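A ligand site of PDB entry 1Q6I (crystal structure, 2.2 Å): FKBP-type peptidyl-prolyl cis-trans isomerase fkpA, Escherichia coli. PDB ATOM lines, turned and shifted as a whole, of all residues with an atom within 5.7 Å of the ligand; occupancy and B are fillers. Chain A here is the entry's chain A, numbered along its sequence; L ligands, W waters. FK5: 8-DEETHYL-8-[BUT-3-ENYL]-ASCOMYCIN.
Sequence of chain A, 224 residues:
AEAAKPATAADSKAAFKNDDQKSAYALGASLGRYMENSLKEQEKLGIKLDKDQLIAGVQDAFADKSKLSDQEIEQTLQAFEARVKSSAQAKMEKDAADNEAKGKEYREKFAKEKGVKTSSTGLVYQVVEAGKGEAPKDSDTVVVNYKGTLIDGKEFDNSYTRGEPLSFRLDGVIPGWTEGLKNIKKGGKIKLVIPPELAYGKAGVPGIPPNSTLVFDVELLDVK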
ATOM      1  N   TYR A 146     -10.611  18.456  -6.742  1.00  0.00           N
ATOM      2  CA  TYR A 146      -9.826  19.381  -5.913  1.00  0.00           C
ATOM      3  C   TYR A 146      -8.643  18.699  -5.241  1.00  0.00           C
ATOM      4  O   TYR A 146      -8.543  17.483  -5.113  1.00  0.00           O
ATOM      5  CB  TYR A 146     -10.708  20.057  -4.848  1.00  0.00           C
ATOM      6  CG  TYR A 146     -11.176  19.106  -3.810  1.00  0.00           C
ATOM      7  CD1 TYR A 146     -12.305  18.364  -4.031  1.00  0.00           C
ATOM      8  CD2 TYR A 146     -10.460  18.894  -2.628  1.00  0.00           C
ATOM      9  CE1 TYR A 146     -12.754  17.444  -3.122  1.00  0.00           C
ATOM     10  CE2 TYR A 146     -10.908  17.957  -1.694  1.00  0.00           C
ATOM     11  CZ  TYR A 146     -12.069  17.227  -1.961  1.00  0.00           C
ATOM     12  OH  TYR A 146     -12.570  16.251  -1.095  1.00  0.00           O
ATOM     13  N   GLY A 148      -6.380  19.575  -1.719  1.00  0.00           N
ATOM     14  CA  GLY A 148      -6.196  20.421  -0.552  1.00  0.00           C
ATOM     15  C   GLY A 148      -4.856  20.187   0.153  1.00  0.00           C
ATOM     16  O   GLY A 148      -4.428  19.035   0.325  1.00  0.00           O
ATOM     17  N   PHE A 156      -3.696  17.123   2.422  1.00  0.00           N
ATOM     18  CA  PHE A 156      -4.593  16.384   3.302  1.00  0.00           C
ATOM     19  C   PHE A 156      -5.709  15.682   2.516  1.00  0.00           C
ATOM     20  O   PHE A 156      -6.301  14.776   3.008  1.00  0.00           O
ATOM     21  CB  PHE A 156      -5.178  17.305   4.407  1.00  0.00           C
ATOM     22  CG  PHE A 156      -5.781  18.584   3.902  1.00  0.00           C
ATOM     23  CD1 PHE A 156      -7.093  18.621   3.535  1.00  0.00           C
ATOM     24  CD2 PHE A 156      -5.046  19.734   3.829  1.00  0.00           C
ATOM     25  CE1 PHE A 156      -7.652  19.760   3.097  1.00  0.00           C
ATOM     26  CE2 PHE A 156      -5.612  20.917   3.380  1.00  0.00           C
ATOM     27  CZ  PHE A 156      -6.901  20.927   3.021  1.00  0.00           C
ATOM     28  N   ASP A 157      -5.997  16.113   1.299  1.00  0.00           N
ATOM     29  CA  ASP A 157      -7.056  15.484   0.490  1.00  0.00           C
ATOM     30  C   ASP A 157      -6.821  15.764  -0.998  1.00  0.00           C
ATOM     31  O   ASP A 157      -6.374  16.850  -1.369  1.00  0.00           O
ATOM     32  CB  ASP A 157      -8.430  15.973   0.970  1.00  0.00           C
ATOM     33  CG  ASP A 157      -9.610  15.167   0.409  1.00  0.00           C
ATOM     34  OD1 ASP A 157      -9.446  14.165  -0.300  1.00  0.00           O
ATOM     35  OD2 ASP A 157     -10.854  15.627   0.742  1.00  0.00           O
ATOM     36  N   ARG A 162      -9.291   9.483  -6.023  1.00  0.00           N
ATOM     37  CA  ARG A 162     -10.416   8.546  -5.889  1.00  0.00           C
ATOM     38  C   ARG A 162     -10.971   8.238  -7.255  1.00  0.00           C
ATOM     39  O   ARG A 162     -11.931   7.499  -7.411  1.00  0.00           O
ATOM     40  CB  ARG A 162     -11.531   9.087  -5.008  1.00  0.00           C
ATOM     41  CG  ARG A 162     -11.165   9.167  -3.532  1.00  0.00           C
ATOM     42  CD  ARG A 162     -12.229   9.842  -2.657  1.00  0.00           C
ATOM     43  NE  ARG A 162     -12.518  11.217  -3.035  1.00  0.00           N
ATOM     44  CZ  ARG A 162     -12.052  12.294  -2.381  1.00  0.00           C
ATOM     45  NH1 ARG A 162     -11.239  12.161  -1.343  1.00  0.00           N
ATOM     46  NH2 ARG A 162     -12.385  13.509  -2.777  1.00  0.00           N
ATOM     47  N   LEU A 166     -16.193  15.044  -6.891  1.00  0.00           N
ATOM     48  CA  LEU A 166     -17.050  15.086  -5.747  1.00  0.00           C
ATOM     49  C   LEU A 166     -18.221  16.017  -6.024  1.00  0.00           C
ATOM     50  O   LEU A 166     -18.060  17.088  -6.549  1.00  0.00           O
ATOM     51  CB  LEU A 166     -16.268  15.646  -4.565  1.00  0.00           C
ATOM     52  CG  LEU A 166     -17.085  15.923  -3.308  1.00  0.00           C
ATOM     53  CD1 LEU A 166     -17.285  14.606  -2.584  1.00  0.00           C
ATOM     54  CD2 LEU A 166     -16.375  16.949  -2.416  1.00  0.00           C
ATOM     55  N   PHE A 168     -21.518  18.043  -4.222  1.00  0.00           N
ATOM     56  CA  PHE A 168     -22.129  18.475  -2.984  1.00  0.00           C
ATOM     57  C   PHE A 168     -22.985  19.742  -3.168  1.00  0.00           C
ATOM     58  O   PHE A 168     -22.849  20.475  -4.173  1.00  0.00           O
ATOM     59  CB  PHE A 168     -21.050  18.749  -1.946  1.00  0.00           C
ATOM     60  CG  PHE A 168     -20.060  19.754  -2.376  1.00  0.00           C
ATOM     61  CD1 PHE A 168     -20.388  21.095  -2.357  1.00  0.00           C
ATOM     62  CD2 PHE A 168     -18.799  19.375  -2.809  1.00  0.00           C
ATOM     63  CE1 PHE A 168     -19.461  22.039  -2.768  1.00  0.00           C
ATOM     64  CE2 PHE A 168     -17.891  20.296  -3.205  1.00  0.00           C
ATOM     65  CZ  PHE A 168     -18.225  21.647  -3.199  1.00  0.00           C
ATOM     66  N   GLY A 172     -23.730  23.461   1.690  1.00  0.00           N
ATOM     67  CA  GLY A 172     -23.457  22.467   2.698  1.00  0.00           C
ATOM     68  C   GLY A 172     -21.993  22.355   3.096  1.00  0.00           C
ATOM     69  O   GLY A 172     -21.666  21.571   4.008  1.00  0.00           O
ATOM     70  N   VAL A 173     -21.122  23.132   2.462  1.00  0.00           N
ATOM     71  CA  VAL A 173     -19.669  23.074   2.692  1.00  0.00           C
ATOM     72  C   VAL A 173     -19.091  24.256   3.505  1.00  0.00           C
ATOM     73  O   VAL A 173     -19.815  25.189   3.885  1.00  0.00           O
ATOM     74  CB  VAL A 173     -18.935  22.964   1.337  1.00  0.00           C
ATOM     75  CG1 VAL A 173     -19.271  21.637   0.661  1.00  0.00           C
ATOM     76  CG2 VAL A 173     -19.260  24.126   0.440  1.00  0.00           C
ATOM     77  N   ILE A 174     -17.807  24.237   3.814  1.00  0.00           N
ATOM     78  CA  ILE A 174     -17.242  25.377   4.564  1.00  0.00           C
ATOM     79  C   ILE A 174     -17.380  26.709   3.797  1.00  0.00           C
ATOM     80  O   ILE A 174     -17.344  26.746   2.534  1.00  0.00           O
ATOM     81  CB  ILE A 174     -15.785  25.126   4.953  1.00  0.00           C
ATOM     82  CG1 ILE A 174     -14.959  24.727   3.745  1.00  0.00           C
ATOM     83  CG2 ILE A 174     -15.682  24.013   5.943  1.00  0.00           C
ATOM     84  CD1 ILE A 174     -13.550  24.952   3.977  1.00  0.00           C
ATOM     85  N   TRP A 177     -15.501  27.860   0.595  1.00  0.00           N
ATOM     86  CA  TRP A 177     -15.849  27.228  -0.677  1.00  0.00           C
ATOM     87  C   TRP A 177     -17.200  27.774  -1.126  1.00  0.00           C
ATOM     88  O   TRP A 177     -17.401  28.028  -2.285  1.00  0.00           O
ATOM     89  CB  TRP A 177     -15.966  25.695  -0.555  1.00  0.00           C
ATOM     90  CG  TRP A 177     -14.732  24.932  -0.715  1.00  0.00           C
ATOM     91  CD1 TRP A 177     -13.670  24.901   0.125  1.00  0.00           C
ATOM     92  CD2 TRP A 177     -14.430  24.036  -1.778  1.00  0.00           C
ATOM     93  NE1 TRP A 177     -12.719  24.045  -0.357  1.00  0.00           N
ATOM     94  CE2 TRP A 177     -13.167  23.490  -1.512  1.00  0.00           C
ATOM     95  CE3 TRP A 177     -15.129  23.609  -2.912  1.00  0.00           C
ATOM     96  CZ2 TRP A 177     -12.547  22.567  -2.366  1.00  0.00           C
ATOM     97  CZ3 TRP A 177     -14.548  22.671  -3.746  1.00  0.00           C
ATOM     98  CH2 TRP A 177     -13.263  22.162  -3.476  1.00  0.00           C
ATOM     99  N   ALA A 199     -13.020  28.191   7.571  1.00  0.00           N
ATOM    100  CA  ALA A 199     -12.764  26.767   7.453  1.00  0.00           C
ATOM    101  C   ALA A 199     -13.094  25.983   8.742  1.00  0.00           C
ATOM    102  O   ALA A 199     -14.248  25.957   9.145  1.00  0.00           O
ATOM    103  CB  ALA A 199     -11.327  26.537   6.979  1.00  0.00           C
ATOM    104  N   TYR A 200     -12.116  25.336   9.368  1.00  0.00           N
ATOM    105  CA  TYR A 200     -12.362  24.508  10.572  1.00  0.00           C
ATOM    106  C   TYR A 200     -11.952  25.161  11.886  1.00  0.00           C
ATOM    107  O   TYR A 200     -11.962  24.528  12.950  1.00  0.00           O
ATOM    108  CB  TYR A 200     -11.703  23.134  10.393  1.00  0.00           C
ATOM    109  CG  TYR A 200     -12.320  22.412   9.201  1.00  0.00           C
ATOM    110  CD1 TYR A 200     -13.545  21.798   9.292  1.00  0.00           C
ATOM    111  CD2 TYR A 200     -11.687  22.425   7.974  1.00  0.00           C
ATOM    112  CE1 TYR A 200     -14.107  21.160   8.178  1.00  0.00           C
ATOM    113  CE2 TYR A 200     -12.223  21.814   6.876  1.00  0.00           C
ATOM    114  CZ  TYR A 200     -13.425  21.173   6.975  1.00  0.00           C
ATOM    115  OH  TYR A 200     -13.963  20.610   5.845  1.00  0.00           O
ATOM    116  N   VAL A 205      -9.901  19.527  12.596  1.00  0.00           N
ATOM    117  CA  VAL A 205     -10.503  18.219  12.532  1.00  0.00           C
ATOM    118  C   VAL A 205      -9.336  17.298  12.228  1.00  0.00           C
ATOM    119  O   VAL A 205      -8.247  17.792  11.968  1.00  0.00           O
ATOM    120  CB  VAL A 205     -11.569  18.100  11.428  1.00  0.00           C
ATOM    121  CG1 VAL A 205     -12.702  19.130  11.637  1.00  0.00           C
ATOM    122  CG2 VAL A 205     -10.962  18.274  10.058  1.00  0.00           C
ATOM    123  N   PRO A 206      -9.541  15.973  12.284  1.00  0.00           N
ATOM    124  CA  PRO A 206      -8.424  15.045  12.029  1.00  0.00           C
ATOM    125  C   PRO A 206      -7.724  15.351  10.719  1.00  0.00           C
ATOM    126  O   PRO A 206      -8.371  15.502   9.660  1.00  0.00           O
ATOM    127  CB  PRO A 206      -9.101  13.671  12.046  1.00  0.00           C
ATOM    128  CG  PRO A 206     -10.263  13.886  13.031  1.00  0.00           C
ATOM    129  CD  PRO A 206     -10.773  15.257  12.646  1.00  0.00           C
ATOM    130  N   ILE A 208      -6.270  18.185  10.117  1.00  0.00           N
ATOM    131  CA  ILE A 208      -6.185  19.625   9.962  1.00  0.00           C
ATOM    132  C   ILE A 208      -6.019  20.318  11.298  1.00  0.00           C
ATOM    133  O   ILE A 208      -6.952  20.477  12.057  1.00  0.00           O
ATOM    134  CB  ILE A 208      -7.392  20.122   9.238  1.00  0.00           C
ATOM    135  CG1 ILE A 208      -7.331  19.523   7.838  1.00  0.00           C
ATOM    136  CG2 ILE A 208      -7.446  21.686   9.259  1.00  0.00           C
ATOM    137  CD1 ILE A 208      -7.985  20.254   6.828  1.00  0.00           C
ATOM    138  N   LEU A 214      -6.193  26.936   4.807  1.00  0.00           N
ATOM    139  CA  LEU A 214      -6.173  25.867   3.812  1.00  0.00           C
ATOM    140  C   LEU A 214      -6.012  26.402   2.402  1.00  0.00           C
ATOM    141  O   LEU A 214      -6.596  27.397   2.057  1.00  0.00           O
ATOM    142  CB  LEU A 214      -7.443  25.020   3.892  1.00  0.00           C
ATOM    143  CG  LEU A 214      -7.906  24.632   5.284  1.00  0.00           C
ATOM    144  CD1 LEU A 214      -9.176  23.799   5.124  1.00  0.00           C
ATOM    145  CD2 LEU A 214      -6.813  23.858   6.094  1.00  0.00           C
ATOM    146  N   PHE A 216      -6.719  25.356  -1.432  1.00  0.00           N
ATOM    147  CA  PHE A 216      -7.369  24.398  -2.314  1.00  0.00           C
ATOM    148  C   PHE A 216      -7.174  24.757  -3.794  1.00  0.00           C
ATOM    149  O   PHE A 216      -7.394  25.922  -4.199  1.00  0.00           O
ATOM    150  CB  PHE A 216      -8.857  24.391  -2.027  1.00  0.00           C
ATOM    151  CG  PHE A 216      -9.237  23.669  -0.777  1.00  0.00           C
ATOM    152  CD1 PHE A 216      -9.383  22.302  -0.778  1.00  0.00           C
ATOM    153  CD2 PHE A 216      -9.486  24.364   0.379  1.00  0.00           C
ATOM    154  CE1 PHE A 216      -9.737  21.645   0.356  1.00  0.00           C
ATOM    155  CE2 PHE A 216      -9.839  23.701   1.494  1.00  0.00           C
ATOM    156  CZ  PHE A 216      -9.978  22.353   1.488  1.00  0.00           C
HETATM  157  C1  FK5 L   1     -15.937  20.617   3.007  1.00  0.00           C
HETATM  158  C2  FK5 L   1     -14.646  20.876   2.283  1.00  0.00           C
HETATM  159  C3  FK5 L   1     -14.487  21.699   1.022  1.00  0.00           C
HETATM  160  C4  FK5 L   1     -15.136  20.863  -0.043  1.00  0.00           C
HETATM  161  C5  FK5 L   1     -14.355  19.558  -0.269  1.00  0.00           C
HETATM  162  C6  FK5 L   1     -14.061  18.789   1.028  1.00  0.00           C
HETATM  163  C8  FK5 L   1     -12.710  19.609   2.909  1.00  0.00           C
HETATM  164  C9  FK5 L   1     -11.841  18.553   2.787  1.00  0.00           C
HETATM  165  C10 FK5 L   1     -11.958  17.367   3.704  1.00  0.00           C
HETATM  166  C11 FK5 L   1     -12.112  17.662   5.199  1.00  0.00           C
HETATM  167  C12 FK5 L   1     -12.475  16.402   5.999  1.00  0.00           C
HETATM  168  C13 FK5 L   1     -13.591  15.618   5.335  1.00  0.00           C
HETATM  169  C14 FK5 L   1     -13.274  15.395   3.869  1.00  0.00           C
HETATM  170  C15 FK5 L   1     -14.359  14.637   3.119  1.00  0.00           C
HETATM  171  C16 FK5 L   1     -14.067  13.159   3.006  1.00  0.00           C
HETATM  172  C17 FK5 L   1     -14.892  12.240   3.903  1.00  0.00           C
HETATM  173  C18 FK5 L   1     -16.131  12.908   4.528  1.00  0.00           C
HETATM  174  C19 FK5 L   1     -17.440  12.596   3.820  1.00  0.00           C
HETATM  175  C20 FK5 L   1     -18.689  12.687   4.589  1.00  0.00           C
HETATM  176  C21 FK5 L   1     -19.930  13.288   4.003  1.00  0.00           C
HETATM  177  C22 FK5 L   1     -19.993  14.791   4.182  1.00  0.00           C
HETATM  178  C23 FK5 L   1     -19.322  15.710   3.199  1.00  0.00           C
HETATM  179  C24 FK5 L   1     -19.344  17.156   3.683  1.00  0.00           C
HETATM  180  C25 FK5 L   1     -18.063  17.766   3.144  1.00  0.00           C
HETATM  181  C26 FK5 L   1     -17.612  19.135   3.634  1.00  0.00           C
HETATM  182  C27 FK5 L   1     -17.740  19.104   5.094  1.00  0.00           C
HETATM  183  C28 FK5 L   1     -18.789  19.925   5.668  1.00  0.00           C
HETATM  184  C29 FK5 L   1     -18.895  20.142   7.123  1.00  0.00           C
HETATM  185  C30 FK5 L   1     -18.340  21.514   7.478  1.00  0.00           C
HETATM  186  C31 FK5 L   1     -18.611  21.863   8.950  1.00  0.00           C
HETATM  187  C32 FK5 L   1     -20.099  21.747   9.170  1.00  0.00           C
HETATM  188  C33 FK5 L   1     -20.585  20.338   8.902  1.00  0.00           C
HETATM  189  C34 FK5 L   1     -20.370  20.050   7.432  1.00  0.00           C
HETATM  190  C35 FK5 L   1     -10.864  18.280   5.788  1.00  0.00           C
HETATM  191  C36 FK5 L   1     -13.920  11.683   4.951  1.00  0.00           C
HETATM  192  C37 FK5 L   1     -17.525  12.226   2.364  1.00  0.00           C
HETATM  193  C38 FK5 L   1     -21.120  12.571   4.637  1.00  0.00           C
HETATM  194  C39 FK5 L   1     -21.973  11.957   3.544  1.00  0.00           C
HETATM  195  C40 FK5 L   1     -22.490  10.593   3.706  1.00  0.00           C
HETATM  196  C41 FK5 L   1     -18.285  17.883   1.655  1.00  0.00           C
HETATM  197  C42 FK5 L   1     -16.790  18.267   5.896  1.00  0.00           C
HETATM  198  C43 FK5 L   1     -14.064  14.333   7.286  1.00  0.00           C
HETATM  199  C44 FK5 L   1     -15.080  14.369   0.854  1.00  0.00           C
HETATM  200  C45 FK5 L   1     -17.059  23.337  10.004  1.00  0.00           C
HETATM  201  N7  FK5 L   1     -13.749  19.749   2.118  1.00  0.00           N
HETATM  202  O1  FK5 L   1     -16.247  19.429   3.249  1.00  0.00           O
HETATM  203  O2  FK5 L   1     -16.827  21.665   3.315  1.00  0.00           O
HETATM  204  O3  FK5 L   1     -12.472  20.521   3.911  1.00  0.00           O
HETATM  205  O4  FK5 L   1     -10.869  18.547   1.789  1.00  0.00           O
HETATM  206  O5  FK5 L   1     -13.138  16.677   3.291  1.00  0.00           O
HETATM  207  O6  FK5 L   1     -10.728  16.650   3.451  1.00  0.00           O
HETATM  208  O7  FK5 L   1     -13.774  14.350   5.905  1.00  0.00           O
HETATM  209  O8  FK5 L   1     -14.418  15.158   1.817  1.00  0.00           O
HETATM  210  O9  FK5 L   1     -20.669  15.409   5.237  1.00  0.00           O
HETATM  211  O10 FK5 L   1     -20.425  17.867   3.157  1.00  0.00           O
HETATM  212  O11 FK5 L   1     -18.229  23.182   9.240  1.00  0.00           O
HETATM  213  O12 FK5 L   1     -20.432  22.124  10.476  1.00  0.00           O
HETATM  214  O   HOH W   1     -21.729  16.723   0.975  1.00  0.00           O
HETATM  215  O   HOH W   2     -22.520  19.386   4.540  1.00  0.00           O
HETATM  216  O   HOH W   3     -14.593  11.634   8.430  1.00  0.00           O
HETATM  217  O   HOH W   4     -11.982  13.425   0.967  1.00  0.00           O
HETATM  218  O   HOH W   5     -19.014  25.068   7.918  1.00  0.00           O
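Water W4 lies within hydrogen-bond range of the side-chain carboxylate of Asp 157, the guanidinium group of Arg 162 and an oxygen (O8) of the ligand. Water W2 bridges the backbone carbonyl oxygen (O) of Gly 172 (2.4 Å) and an oxygen (O10) of the ligand (2.9 Å).
The side-chain hydroxyl of Tyr 146 is in hydrogen-bond range of the side-chain carboxylate of Asp 157, 2.6 Å away. The side-chain carboxylate (OD1) of Asp 157 lies within salt-bridge range of the guanidinium group (NH1) of Arg 162. The backbone carbonyl oxygen (O) of Asp 157 lies within hydrogen-bond range of the backbone NH (N) of Gly 148 (2.7 Å). The guanidinium group of Arg 162 lies within hydrogen-bond range of the side-chain hydroxyl of Tyr 146. N of Phe 156 lies within hydrogen-bond range of O of Gly 148, 2.9 Å away.
CE2 of Tyr 146 touches O4 of the ligand, at 3.5 Å. Phe 156 touches the ligand. Leu 166 touches the ligand (CD2 to C5, 3.9 Å). Gly 172 touches the ligand. Val 173 touches the ligand. Trp 177 touches the ligand. Ala 199 touches the ligand (O to C45, 3.9 Å). Ile 208 touches the ligand. CE1 of Phe 216 touches O4 of the ligand (3.6 Å). Hydrophobic or aromatic side chains that line the ligand: Tyr 146, Phe 156, Leu 166, Val 173, Ile 174, Trp 177, Tyr 200, Ile 208 and Phe 216. The nearest printed residue that does not touch the ligand is Phe 168 (4.2 Å).
An oxygen (O3) of the ligand is in hydrogen-bond range of the side-chain hydroxyl (OH) of Tyr 200 (2.4 Å). The backbone NH (N) of Ile 174 lies within hydrogen-bond range of an oxygen (O2) of the ligand (2.8 Å). The side-chain carboxylate of Asp 157 is in hydrogen-bond range of an oxygen (O6) of the ligand.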
